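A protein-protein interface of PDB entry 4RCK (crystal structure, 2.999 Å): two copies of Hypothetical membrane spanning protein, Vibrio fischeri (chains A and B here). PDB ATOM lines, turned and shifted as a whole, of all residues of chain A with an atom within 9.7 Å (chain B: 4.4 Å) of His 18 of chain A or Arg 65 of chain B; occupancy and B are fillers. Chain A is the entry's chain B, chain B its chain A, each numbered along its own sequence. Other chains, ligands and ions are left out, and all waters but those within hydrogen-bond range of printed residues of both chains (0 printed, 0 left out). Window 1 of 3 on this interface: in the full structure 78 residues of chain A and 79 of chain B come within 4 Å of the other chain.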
ATOM      1  N   GLU A  17      16.915 -15.998  -7.912  1.00  0.00           N
ATOM      2  CA  GLU A  17      15.479 -15.876  -7.683  1.00  0.00           C
ATOM      3  C   GLU A  17      15.220 -15.196  -6.345  1.00  0.00           C
ATOM      4  O   GLU A  17      16.125 -15.073  -5.518  1.00  0.00           O
ATOM      5  CB  GLU A  17      14.803 -17.248  -7.731  1.00  0.00           C
ATOM      6  CG  GLU A  17      14.926 -17.972  -9.073  1.00  0.00           C
ATOM      7  CD  GLU A  17      16.292 -18.604  -9.286  1.00  0.00           C
ATOM      8  OE1 GLU A  17      17.144 -18.512  -8.377  1.00  0.00           O
ATOM      9  OE2 GLU A  17      16.513 -19.196 -10.364  1.00  0.00           O
ATOM     10  N   HIS A  18      13.984 -14.755  -6.131  1.00  0.00           N
ATOM     11  CA  HIS A  18      13.658 -13.988  -4.932  1.00  0.00           C
ATOM     12  C   HIS A  18      12.442 -14.542  -4.191  1.00  0.00           C
ATOM     13  O   HIS A  18      11.528 -15.096  -4.801  1.00  0.00           O
ATOM     14  CB  HIS A  18      13.420 -12.520  -5.295  1.00  0.00           C
ATOM     15  CG  HIS A  18      11.992 -12.184  -5.564  1.00  0.00           C
ATOM     16  ND1 HIS A  18      11.185 -11.547  -4.641  1.00  0.00           N
ATOM     17  CD2 HIS A  18      11.208 -12.392  -6.653  1.00  0.00           C
ATOM     18  CE1 HIS A  18       9.981 -11.377  -5.146  1.00  0.00           C
ATOM     19  NE2 HIS A  18       9.969 -11.884  -6.372  1.00  0.00           N
ATOM     20  N   ARG A  19      12.443 -14.390  -2.870  1.00  0.00           N
ATOM     21  CA  ARG A  19      11.337 -14.851  -2.038  1.00  0.00           C
ATOM     22  C   ARG A  19      10.690 -13.698  -1.277  1.00  0.00           C
ATOM     23  O   ARG A  19      11.330 -12.685  -1.001  1.00  0.00           O
ATOM     24  CB  ARG A  19      11.813 -15.911  -1.044  1.00  0.00           C
ATOM     25  CG  ARG A  19      13.242 -16.358  -1.231  1.00  0.00           C
ATOM     26  CD  ARG A  19      13.688 -17.236  -0.080  1.00  0.00           C
ATOM     27  NE  ARG A  19      13.052 -18.548  -0.087  1.00  0.00           N
ATOM     28  CZ  ARG A  19      13.551 -19.604  -0.717  1.00  0.00           C
ATOM     29  NH1 ARG A  19      14.685 -19.487  -1.398  1.00  0.00           N
ATOM     30  NH2 ARG A  19      12.920 -20.768  -0.673  1.00  0.00           N
ATOM     31  N   ASP A  20       9.412 -13.854  -0.949  1.00  0.00           N
ATOM     32  CA  ASP A  20       8.725 -12.909  -0.076  1.00  0.00           C
ATOM     33  C   ASP A  20       8.634 -13.488   1.328  1.00  0.00           C
ATOM     34  O   ASP A  20       8.104 -14.581   1.522  1.00  0.00           O
ATOM     35  CB  ASP A  20       7.329 -12.579  -0.606  1.00  0.00           C
ATOM     36  CG  ASP A  20       7.367 -11.656  -1.806  1.00  0.00           C
ATOM     37  OD1 ASP A  20       8.453 -11.496  -2.400  1.00  0.00           O
ATOM     38  OD2 ASP A  20       6.307 -11.096  -2.158  1.00  0.00           O
ATOM     39  N   MET A  21       9.151 -12.756   2.309  1.00  0.00           N
ATOM     40  CA  MET A  21       9.253 -13.292   3.658  1.00  0.00           C
ATOM     41  C   MET A  21       8.638 -12.380   4.708  1.00  0.00           C
ATOM     42  O   MET A  21       9.004 -11.211   4.832  1.00  0.00           O
ATOM     43  CB  MET A  21      10.715 -13.570   3.992  1.00  0.00           C
ATOM     44  CG  MET A  21      11.389 -14.446   2.956  1.00  0.00           C
ATOM     45  SD  MET A  21      13.261 -14.748   3.313  1.00  0.00           S
ATOM     46  CE  MET A  21      13.081 -15.876   4.891  1.00  0.00           C
ATOM     47  N   ARG A  61      19.315 -11.022   3.829  1.00  0.00           N
ATOM     48  CA  ARG A  61      18.489 -11.296   2.651  1.00  0.00           C
ATOM     49  C   ARG A  61      18.480 -10.114   1.690  1.00  0.00           C
ATOM     50  O   ARG A  61      17.584  -9.270   1.729  1.00  0.00           O
ATOM     51  CB  ARG A  61      17.070 -11.641   3.078  1.00  0.00           C
ATOM     52  CG  ARG A  61      17.021 -12.613   4.239  1.00  0.00           C
ATOM     53  CD  ARG A  61      16.454 -13.943   3.819  1.00  0.00           C
ATOM     54  NE  ARG A  61      17.457 -14.968   3.556  1.00  0.00           N
ATOM     55  CZ  ARG A  61      17.252 -15.996   2.739  1.00  0.00           C
ATOM     56  NH1 ARG A  61      16.090 -16.107   2.107  1.00  0.00           N
ATOM     57  NH2 ARG A  61      18.202 -16.900   2.545  1.00  0.00           N
ATOM     58  N   LYS A  62      19.487 -10.076   0.825  1.00  0.00           N
ATOM     59  CA  LYS A  62      19.717  -8.948  -0.065  1.00  0.00           C
ATOM     60  C   LYS A  62      18.633  -8.806  -1.129  1.00  0.00           C
ATOM     61  O   LYS A  62      18.163  -7.700  -1.403  1.00  0.00           O
ATOM     62  CB  LYS A  62      21.084  -9.088  -0.744  1.00  0.00           C
ATOM     63  CG  LYS A  62      22.266  -9.218   0.213  1.00  0.00           C
ATOM     64  CD  LYS A  62      23.036  -7.909   0.347  1.00  0.00           C
ATOM     65  CE  LYS A  62      23.586  -7.434  -0.996  1.00  0.00           C
ATOM     66  NZ  LYS A  62      24.573  -8.385  -1.581  1.00  0.00           N
ATOM     67  N   GLY A  63      18.237  -9.924  -1.726  1.00  0.00           N
ATOM     68  CA  GLY A  63      17.359  -9.882  -2.881  1.00  0.00           C
ATOM     69  C   GLY A  63      15.894 -10.165  -2.614  1.00  0.00           C
ATOM     70  O   GLY A  63      15.138 -10.431  -3.549  1.00  0.00           O
ATOM     71  N   ASP A  64      15.477 -10.093  -1.353  1.00  0.00           N
ATOM     72  CA  ASP A  64      14.139 -10.559  -0.997  1.00  0.00           C
ATOM     73  C   ASP A  64      13.247  -9.495  -0.372  1.00  0.00           C
ATOM     74  O   ASP A  64      13.723  -8.533   0.233  1.00  0.00           O
ATOM     75  CB  ASP A  64      14.250 -11.754  -0.049  1.00  0.00           C
ATOM     76  CG  ASP A  64      14.916 -12.954  -0.704  1.00  0.00           C
ATOM     77  OD1 ASP A  64      15.987 -13.392  -0.221  1.00  0.00           O
ATOM     78  OD2 ASP A  64      14.365 -13.471  -1.699  1.00  0.00           O
ATOM     79  N   ARG A  65      11.941  -9.691  -0.519  1.00  0.00           N
ATOM     80  CA  ARG A  65      10.965  -8.806   0.091  1.00  0.00           C
ATOM     81  C   ARG A  65      10.703  -9.224   1.530  1.00  0.00           C
ATOM     82  O   ARG A  65      10.464 -10.398   1.814  1.00  0.00           O
ATOM     83  CB  ARG A  65       9.659  -8.801  -0.705  1.00  0.00           C
ATOM     84  CG  ARG A  65       9.687  -7.947  -1.962  1.00  0.00           C
ATOM     85  CD  ARG A  65       8.290  -7.475  -2.334  1.00  0.00           C
ATOM     86  NE  ARG A  65       7.420  -8.560  -2.774  1.00  0.00           N
ATOM     87  CZ  ARG A  65       6.336  -8.374  -3.518  1.00  0.00           C
ATOM     88  NH1 ARG A  65       5.592  -9.407  -3.885  1.00  0.00           N
ATOM     89  NH2 ARG A  65       6.003  -7.152  -3.905  1.00  0.00           N
ATOM     90  N   LEU A  66      10.753  -8.255   2.436  1.00  0.00           N
ATOM     91  CA  LEU A  66      10.457  -8.508   3.837  1.00  0.00           C
ATOM     92  C   LEU A  66       9.414  -7.530   4.353  1.00  0.00           C
ATOM     93  O   LEU A  66       9.391  -6.362   3.963  1.00  0.00           O
ATOM     94  CB  LEU A  66      11.726  -8.422   4.689  1.00  0.00           C
ATOM     95  CG  LEU A  66      12.728  -9.570   4.537  1.00  0.00           C
ATOM     96  CD1 LEU A  66      13.692  -9.321   3.386  1.00  0.00           C
ATOM     97  CD2 LEU A  66      13.480  -9.790   5.835  1.00  0.00           C
ATOM     98  N   LEU A  81       5.874  -5.457   3.236  1.00  0.00           N
ATOM     99  CA  LEU A  81       6.646  -6.231   2.261  1.00  0.00           C
ATOM    100  C   LEU A  81       7.488  -5.429   1.273  1.00  0.00           C
ATOM    101  O   LEU A  81       7.401  -5.650   0.065  1.00  0.00           O
ATOM    102  CB  LEU A  81       5.705  -7.131   1.458  1.00  0.00           C
ATOM    103  CG  LEU A  81       5.777  -8.630   1.749  1.00  0.00           C
ATOM    104  CD1 LEU A  81       5.103  -9.421   0.636  1.00  0.00           C
ATOM    105  CD2 LEU A  81       7.210  -9.095   1.961  1.00  0.00           C
ATOM    106  N   THR A  82       8.318  -4.523   1.767  1.00  0.00           N
ATOM    107  CA  THR A  82       9.180  -3.767   0.873  1.00  0.00           C
ATOM    108  C   THR A  82      10.460  -4.538   0.550  1.00  0.00           C
ATOM    109  O   THR A  82      10.878  -5.413   1.311  1.00  0.00           O
ATOM    110  CB  THR A  82       9.538  -2.404   1.474  1.00  0.00           C
ATOM    111  OG1 THR A  82      10.834  -2.012   1.018  1.00  0.00           O
ATOM    112  CG2 THR A  82       9.567  -2.487   2.972  1.00  0.00           C
ATOM    113  N   PHE A  83      11.052  -4.227  -0.601  1.00  0.00           N
ATOM    114  CA  PHE A  83      12.375  -4.725  -0.966  1.00  0.00           C
ATOM    115  C   PHE A  83      13.412  -4.014  -0.109  1.00  0.00           C
ATOM    116  O   PHE A  83      14.400  -4.607   0.321  1.00  0.00           O
ATOM    117  CB  PHE A  83      12.668  -4.483  -2.451  1.00  0.00           C
ATOM    118  CG  PHE A  83      12.227  -5.599  -3.367  1.00  0.00           C
ATOM    119  CD1 PHE A  83      12.956  -6.778  -3.459  1.00  0.00           C
ATOM    120  CD2 PHE A  83      11.110  -5.452  -4.173  1.00  0.00           C
ATOM    121  CE1 PHE A  83      12.558  -7.799  -4.311  1.00  0.00           C
ATOM    122  CE2 PHE A  83      10.712  -6.470  -5.026  1.00  0.00           C
ATOM    123  CZ  PHE A  83      11.440  -7.640  -5.097  1.00  0.00           C
ATOM    124  N   PHE A 117       0.516 -11.084   1.953  1.00  0.00           N
ATOM    125  CA  PHE A 117       1.143 -11.668   0.775  1.00  0.00           C
ATOM    126  C   PHE A 117       0.295 -11.368  -0.455  1.00  0.00           C
ATOM    127  O   PHE A 117       0.811 -11.205  -1.562  1.00  0.00           O
ATOM    128  CB  PHE A 117       1.312 -13.179   0.939  1.00  0.00           C
ATOM    129  CG  PHE A 117       2.501 -13.574   1.766  1.00  0.00           C
ATOM    130  CD1 PHE A 117       3.751 -13.033   1.515  1.00  0.00           C
ATOM    131  CD2 PHE A 117       2.367 -14.491   2.795  1.00  0.00           C
ATOM    132  CE1 PHE A 117       4.846 -13.402   2.274  1.00  0.00           C
ATOM    133  CE2 PHE A 117       3.456 -14.861   3.558  1.00  0.00           C
ATOM    134  CZ  PHE A 117       4.696 -14.317   3.299  1.00  0.00           C
ATOM    135  N   SER A 120      -0.266  -7.454  -2.006  1.00  0.00           N
ATOM    136  CA  SER A 120       0.950  -6.906  -2.596  1.00  0.00           C
ATOM    137  C   SER A 120       0.697  -6.336  -3.989  1.00  0.00           C
ATOM    138  O   SER A 120       1.346  -5.375  -4.402  1.00  0.00           O
ATOM    139  CB  SER A 120       2.039  -7.978  -2.662  1.00  0.00           C
ATOM    140  OG  SER A 120       1.551  -9.156  -3.278  1.00  0.00           O
ATOM    141  N   PRO A 123       5.002  -5.543  -8.894  1.00  0.00           N
ATOM    142  CA  PRO A 123       5.826  -4.427  -9.373  1.00  0.00           C
ATOM    143  C   PRO A 123       5.471  -3.999 -10.795  1.00  0.00           C
ATOM    144  O   PRO A 123       5.027  -4.824 -11.595  1.00  0.00           O
ATOM    145  CB  PRO A 123       7.246  -4.994  -9.318  1.00  0.00           C
ATOM    146  CG  PRO A 123       7.066  -6.470  -9.429  1.00  0.00           C
ATOM    147  CD  PRO A 123       5.805  -6.757  -8.668  1.00  0.00           C
ATOM    148  N   GLN A 124       5.657  -2.718 -11.097  1.00  0.00           N
ATOM    149  CA  GLN A 124       5.404  -2.194 -12.434  1.00  0.00           C
ATOM    150  C   GLN A 124       6.406  -2.762 -13.432  1.00  0.00           C
ATOM    151  O   GLN A 124       7.577  -2.962 -13.102  1.00  0.00           O
ATOM    152  CB  GLN A 124       5.462  -0.667 -12.430  1.00  0.00           C
ATOM    153  CG  GLN A 124       4.246   0.001 -11.810  1.00  0.00           C
ATOM    154  CD  GLN A 124       3.145   0.260 -12.818  1.00  0.00           C
ATOM    155  OE1 GLN A 124       2.582  -0.668 -13.397  1.00  0.00           O
ATOM    156  NE2 GLN A 124       2.840   1.533 -13.042  1.00  0.00           N
ATOM    157  N   ARG A 125       5.942  -3.019 -14.651  1.00  0.00           N
ATOM    158  CA  ARG A 125       6.772  -3.657 -15.667  1.00  0.00           C
ATOM    159  C   ARG A 125       6.995  -2.772 -16.887  1.00  0.00           C
ATOM    160  O   ARG A 125       6.075  -2.103 -17.357  1.00  0.00           O
ATOM    161  CB  ARG A 125       6.145  -4.982 -16.099  1.00  0.00           C
ATOM    162  CG  ARG A 125       6.409  -6.125 -15.142  1.00  0.00           C
ATOM    163  CD  ARG A 125       5.248  -7.097 -15.120  1.00  0.00           C
ATOM    164  NE  ARG A 125       5.635  -8.392 -14.571  1.00  0.00           N
ATOM    165  CZ  ARG A 125       4.778  -9.361 -14.269  1.00  0.00           C
ATOM    166  NH1 ARG A 125       3.477  -9.179 -14.452  1.00  0.00           N
ATOM    167  NH2 ARG A 125       5.221 -10.510 -13.779  1.00  0.00           N
ATOM    168  N   THR A 126       8.223  -2.777 -17.398  1.00  0.00           N
ATOM    169  CA  THR A 126       8.559  -2.009 -18.591  1.00  0.00           C
ATOM    170  C   THR A 126       9.597  -2.700 -19.466  1.00  0.00           C
ATOM    171  O   THR A 126      10.551  -3.301 -18.973  1.00  0.00           O
ATOM    172  CB  THR A 126       9.089  -0.608 -18.235  1.00  0.00           C
ATOM    173  OG1 THR A 126       9.710  -0.641 -16.944  1.00  0.00           O
ATOM    174  CG2 THR A 126       7.954   0.402 -18.219  1.00  0.00           C
ATOM    175  N   ILE A 127       9.393  -2.605 -20.774  1.00  0.00           N
ATOM    176  CA  ILE A 127      10.362  -3.081 -21.748  1.00  0.00           C
ATOM    177  C   ILE A 127      10.950  -1.891 -22.491  1.00  0.00           C
ATOM    178  O   ILE A 127      10.217  -1.003 -22.919  1.00  0.00           O
ATOM    179  CB  ILE A 127       9.726  -4.046 -22.771  1.00  0.00           C
ATOM    180  CG1 ILE A 127       8.952  -5.162 -22.066  1.00  0.00           C
ATOM    181  CG2 ILE A 127      10.793  -4.614 -23.703  1.00  0.00           C
ATOM    182  CD1 ILE A 127       9.796  -6.367 -21.730  1.00  0.00           C
ATOM    183  N   ILE A 128      12.270  -1.861 -22.631  1.00  0.00           N
ATOM    184  CA  ILE A 128      12.897  -0.870 -23.495  1.00  0.00           C
ATOM    185  C   ILE A 128      13.617  -1.581 -24.635  1.00  0.00           C
ATOM    186  O   ILE A 128      14.664  -2.199 -24.439  1.00  0.00           O
ATOM    187  CB  ILE A 128      13.873   0.034 -22.729  1.00  0.00           C
ATOM    188  CG1 ILE A 128      13.170   0.662 -21.522  1.00  0.00           C
ATOM    189  CG2 ILE A 128      14.417   1.119 -23.647  1.00  0.00           C
ATOM    190  CD1 ILE A 128      14.015   1.663 -20.768  1.00  0.00           C
ATOM    191  N   ARG B  19       9.992  -1.017  -9.473  1.00  0.00           N
ATOM    192  CA  ARG B  19       9.687  -1.393 -10.853  1.00  0.00           C
ATOM    193  C   ARG B  19      10.531  -2.563 -11.357  1.00  0.00           C
ATOM    194  O   ARG B  19      11.664  -2.757 -10.922  1.00  0.00           O
ATOM    195  CB  ARG B  19       9.890  -0.197 -11.788  1.00  0.00           C
ATOM    196  CG  ARG B  19       8.823   0.876 -11.705  1.00  0.00           C
ATOM    197  CD  ARG B  19       9.099   1.983 -12.710  1.00  0.00           C
ATOM    198  NE  ARG B  19       7.878   2.466 -13.346  1.00  0.00           N
ATOM    199  CZ  ARG B  19       7.132   3.460 -12.877  1.00  0.00           C
ATOM    200  NH1 ARG B  19       7.481   4.083 -11.761  1.00  0.00           N
ATOM    201  NH2 ARG B  19       6.037   3.831 -13.526  1.00  0.00           N
ATOM    202  N   ASP B  20       9.964  -3.334 -12.280  1.00  0.00           N
ATOM    203  CA  ASP B  20      10.705  -4.359 -13.012  1.00  0.00           C
ATOM    204  C   ASP B  20      10.870  -3.934 -14.464  1.00  0.00           C
ATOM    205  O   ASP B  20       9.887  -3.801 -15.189  1.00  0.00           O
ATOM    206  CB  ASP B  20       9.996  -5.714 -12.944  1.00  0.00           C
ATOM    207  CG  ASP B  20      10.239  -6.434 -11.636  1.00  0.00           C
ATOM    208  OD1 ASP B  20      11.176  -6.044 -10.908  1.00  0.00           O
ATOM    209  OD2 ASP B  20       9.500  -7.398 -11.342  1.00  0.00           O
ATOM    210  N   MET B  21      12.108  -3.721 -14.892  1.00  0.00           N
ATOM    211  CA  MET B  21      12.348  -3.232 -16.243  1.00  0.00           C
ATOM    212  C   MET B  21      13.332  -4.113 -17.002  1.00  0.00           C
ATOM    213  O   MET B  21      14.457  -4.337 -16.555  1.00  0.00           O
ATOM    214  CB  MET B  21      12.850  -1.788 -16.202  1.00  0.00           C
ATOM    215  CG  MET B  21      12.736  -1.136 -14.833  1.00  0.00           C
ATOM    216  SD  MET B  21      12.305   0.757 -14.948  1.00  0.00           S
ATOM    217  CE  MET B  21      13.527   1.233 -16.387  1.00  0.00           C
ATOM    218  N   ASP B  64      14.721  -0.235  -8.367  1.00  0.00           N
ATOM    219  CA  ASP B  64      14.083  -1.079  -9.373  1.00  0.00           C
ATOM    220  C   ASP B  64      14.964  -2.260  -9.765  1.00  0.00           C
ATOM    221  O   ASP B  64      16.187  -2.201  -9.646  1.00  0.00           O
ATOM    222  CB  ASP B  64      13.738  -0.257 -10.617  1.00  0.00           C
ATOM    223  CG  ASP B  64      13.070   1.061 -10.279  1.00  0.00           C
ATOM    224  OD1 ASP B  64      11.981   1.037  -9.670  1.00  0.00           O
ATOM    225  OD2 ASP B  64      13.631   2.120 -10.631  1.00  0.00           O
ATOM    226  N   ARG B  65      14.332  -3.336 -10.228  1.00  0.00           N
ATOM    227  CA  ARG B  65      15.063  -4.473 -10.775  1.00  0.00           C
ATOM    228  C   ARG B  65      15.261  -4.314 -12.274  1.00  0.00           C
ATOM    229  O   ARG B  65      14.364  -3.864 -12.985  1.00  0.00           O
ATOM    230  CB  ARG B  65      14.339  -5.789 -10.487  1.00  0.00           C
ATOM    231  CG  ARG B  65      14.677  -6.401  -9.146  1.00  0.00           C
ATOM    232  CD  ARG B  65      14.097  -7.796  -9.014  1.00  0.00           C
ATOM    233  NE  ARG B  65      12.656  -7.809  -9.237  1.00  0.00           N
ATOM    234  CZ  ARG B  65      11.933  -8.915  -9.366  1.00  0.00           C
ATOM    235  NH1 ARG B  65      12.519 -10.103  -9.296  1.00  0.00           N
ATOM    236  NH2 ARG B  65      10.626  -8.836  -9.568  1.00  0.00           N
ATOM    237  N   LEU B  66      16.441  -4.692 -12.750  1.00  0.00           N
ATOM    238  CA  LEU B  66      16.769  -4.567 -14.163  1.00  0.00           C
ATOM    239  C   LEU B  66      17.352  -5.864 -14.717  1.00  0.00           C
ATOM    240  O   LEU B  66      18.090  -6.571 -14.029  1.00  0.00           O
ATOM    241  CB  LEU B  66      17.746  -3.408 -14.377  1.00  0.00           C
ATOM    242  CG  LEU B  66      17.152  -2.004 -14.241  1.00  0.00           C
ATOM    243  CD1 LEU B  66      18.238  -0.968 -14.001  1.00  0.00           C
ATOM    244  CD2 LEU B  66      16.352  -1.653 -15.484  1.00  0.00           C
ATOM    245  N   LEU B  81      17.451 -10.694 -13.678  1.00  0.00           N
ATOM    246  CA  LEU B  81      16.871  -9.498 -13.065  1.00  0.00           C
ATOM    247  C   LEU B  81      17.606  -9.314 -11.745  1.00  0.00           C
ATOM    248  O   LEU B  81      18.000 -10.299 -11.123  1.00  0.00           O
ATOM    249  CB  LEU B  81      15.359  -9.629 -12.831  1.00  0.00           C
ATOM    250  CG  LEU B  81      14.368  -9.007 -13.827  1.00  0.00           C
ATOM    251  CD1 LEU B  81      12.955  -9.492 -13.549  1.00  0.00           C
ATOM    252  CD2 LEU B  81      14.423  -7.489 -13.810  1.00  0.00           C
ATOM    253  N   THR B  82      17.791  -8.072 -11.309  1.00  0.00           N
ATOM    254  CA  THR B  82      18.581  -7.825 -10.104  1.00  0.00           C
ATOM    255  C   THR B  82      18.476  -6.418  -9.539  1.00  0.00           C
ATOM    256  O   THR B  82      18.035  -5.486 -10.208  1.00  0.00           O
ATOM    257  CB  THR B  82      20.075  -8.087 -10.358  1.00  0.00           C
ATOM    258  OG1 THR B  82      20.836  -7.662  -9.221  1.00  0.00           O
ATOM    259  CG2 THR B  82      20.534  -7.316 -11.576  1.00  0.00           C
ATOM    260  N   PHE B  83      18.909  -6.281  -8.291  1.00  0.00           N
ATOM    261  CA  PHE B  83      19.007  -4.986  -7.638  1.00  0.00           C
ATOM    262  C   PHE B  83      20.415  -4.441  -7.767  1.00  0.00           C
ATOM    263  O   PHE B  83      20.681  -3.275  -7.469  1.00  0.00           O
ATOM    264  CB  PHE B  83      18.615  -5.093  -6.168  1.00  0.00           C
ATOM    265  CG  PHE B  83      17.180  -4.778  -5.911  1.00  0.00           C
ATOM    266  CD1 PHE B  83      16.815  -3.532  -5.444  1.00  0.00           C
ATOM    267  CD2 PHE B  83      16.196  -5.717  -6.148  1.00  0.00           C
ATOM    268  CE1 PHE B  83      15.493  -3.226  -5.206  1.00  0.00           C
ATOM    269  CE2 PHE B  83      14.877  -5.419  -5.909  1.00  0.00           C
ATOM    270  CZ  PHE B  83      14.523  -4.170  -5.442  1.00  0.00           C
ATOM    271  N   SER B 120       9.354 -13.881 -12.131  1.00  0.00           N
ATOM    272  CA  SER B 120       9.148 -12.999 -10.987  1.00  0.00           C
ATOM    273  C   SER B 120       7.708 -13.129 -10.503  1.00  0.00           C
ATOM    274  O   SER B 120       7.311 -12.498  -9.522  1.00  0.00           O
ATOM    275  CB  SER B 120       9.463 -11.544 -11.345  1.00  0.00           C
ATOM    276  OG  SER B 120       8.401 -10.952 -12.075  1.00  0.00           O
ATOM    277  N   PRO B 123       7.206 -16.062  -6.481  1.00  0.00           N
ATOM    278  CA  PRO B 123       8.057 -16.009  -5.292  1.00  0.00           C
ATOM    279  C   PRO B 123       7.617 -17.045  -4.269  1.00  0.00           C
ATOM    280  O   PRO B 123       6.418 -17.271  -4.107  1.00  0.00           O
ATOM    281  CB  PRO B 123       7.845 -14.583  -4.759  1.00  0.00           C
ATOM    282  CG  PRO B 123       6.737 -13.971  -5.607  1.00  0.00           C
ATOM    283  CD  PRO B 123       6.121 -15.070  -6.412  1.00  0.00           C
ATOM    284  N   GLN B 124       8.571 -17.672  -3.592  1.00  0.00           N
ATOM    285  CA  GLN B 124       8.231 -18.626  -2.548  1.00  0.00           C
ATOM    286  C   GLN B 124       7.977 -17.888  -1.241  1.00  0.00           C
ATOM    287  O   GLN B 124       8.787 -17.069  -0.808  1.00  0.00           O
ATOM    288  CB  GLN B 124       9.333 -19.672  -2.386  1.00  0.00           C
ATOM    289  CG  GLN B 124       9.426 -20.622  -3.568  1.00  0.00           C
ATOM    290  CD  GLN B 124      10.569 -21.608  -3.446  1.00  0.00           C
ATOM    291  OE1 GLN B 124      10.977 -21.972  -2.344  1.00  0.00           O
ATOM    292  NE2 GLN B 124      11.094 -22.044  -4.585  1.00  0.00           N
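His 18 of chain A touches just these residues of chain B: Arg 65 (3.7 Å) and Pro 123 (3.6 Å).
Of the printed residues of chain B, Asp 20 of chain A touches Pro 123 (3.9 Å) and Gln 124 (3.3 Å).
Of the printed residues of chain B, Arg 125 of chain A touches Asp 20 (3.2 Å) and Ser 120 (3.6 Å).
Of the printed residues of chain B, Thr 126 of chain A touches Asp 20 (2.9 Å) and Met 21 (3.3 Å).
Printed residues of chain A within 4 Å of Arg 65 of chain B: His 18.
No residue of chain A comes within 4 Å of Leu 66 of chain B.
Printed residues of chain A within 4 Å of Phe 83 of chain B: Phe 83 (3.4 Å).
The nearest residue of chain B that does not touch His 18 of chain A is Gln 124 of chain B (4.1 Å).
The nearest printed residue of chain B that does not touch Phe 83 of chain A is Arg 65 of chain B (4.3 Å).
Arg 19 of chain A touches Gln 124 of chain B, and with the chains exchanged Gln 124 of chain A touches Arg 19 of chain B.
Asp 20 of chain A touches Pro 123 of chain B, and with the chains exchanged Pro 123 of chain A touches Asp 20 of chain B.
Asp 20 of chain A touches Gln 124 of chain B, and with the chains exchanged Gln 124 of chain A touches Asp 20 of chain B.
Phe 83 of chain B touches its own counterpart, Phe 83 of chain A.
12 positions are printed for both chains.
Of the 13 pairs that touch across the chains among the printed residues, 7 have their exchanged pair printed and touching as well.
His 18 of chain A touches Arg 65 of chain B.
His 18 of chain A touches Pro 123 of chain B (O to CA, 3.6 Å).
Asp 20 of chain A touches Pro 123 of chain B.
CE2 of Phe 83 of chain B touches CD1 of Phe 83 of chain A, 3.4 Å away.
Pro 123 of chain A touches Asp 20 of chain B (CG to OD2, 3.2 Å).
Gln 124 of chain A touches Arg 19 of chain B (O to C, 3.5 Å).
Asp 20 of chain B touches Arg 125 of chain A (O to CA, 3.2 Å).
Ser 120 of chain B touches Arg 125 of chain A (OG to NH2, 3.6 Å).
The backbone NH (N) of Asp 20 of chain B sits at hydrogen-bond distance from the backbone carbonyl oxygen (O) of Gln 124 of chain A (2.6 Å).
The backbone carbonyl oxygen of Asp 20 of chain B lies within hydrogen-bond range of the backbone NH of Thr 126 of chain A, at 2.9 Å.
OG1 of Thr 126 of chain A sits close to SD of Met 21 of chain B.
OE1 of Gln 124 of chain B lies within hydrogen-bond range of NH2 of Arg 19 of chain A (2.8 Å).
The backbone carbonyl oxygen (O) of Gln 124 of chain B sits at hydrogen-bond distance from the backbone NH (N) of Asp 20 of chain A.
The side-chain carboxylate (OD2) of Asp 20 of chain A is in salt-bridge range of the guanidinium group (NH1) of Arg 65 of chain A, 2.5 Å away.
OD1 of Asp 64 of chain B is in hydrogen-bond range of N of Arg 19 of chain B, at 2.9 Å.
The side-chain carboxylate (OD2) of Asp 20 of chain B lies within salt-bridge range of the guanidinium group (NH2) of Arg 65 of chain B (2.5 Å).
O of Arg 19 of chain B sits at hydrogen-bond distance from N of Arg 65 of chain B, at 2.8 Å.
The backbone NH of Arg 65 of chain A sits at hydrogen-bond distance from the backbone carbonyl oxygen of Arg 19 of chain A (3.1 Å).
OD2 of Asp 64 of chain A sits at hydrogen-bond distance from N of Arg 19 of chain A, 2.4 Å away.
Of the 12 printed residues of chain B, 8 touch a printed residue of chain A.
Along chain B the printed residues that touch a printed residue of chain A span positions 19 to 124.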
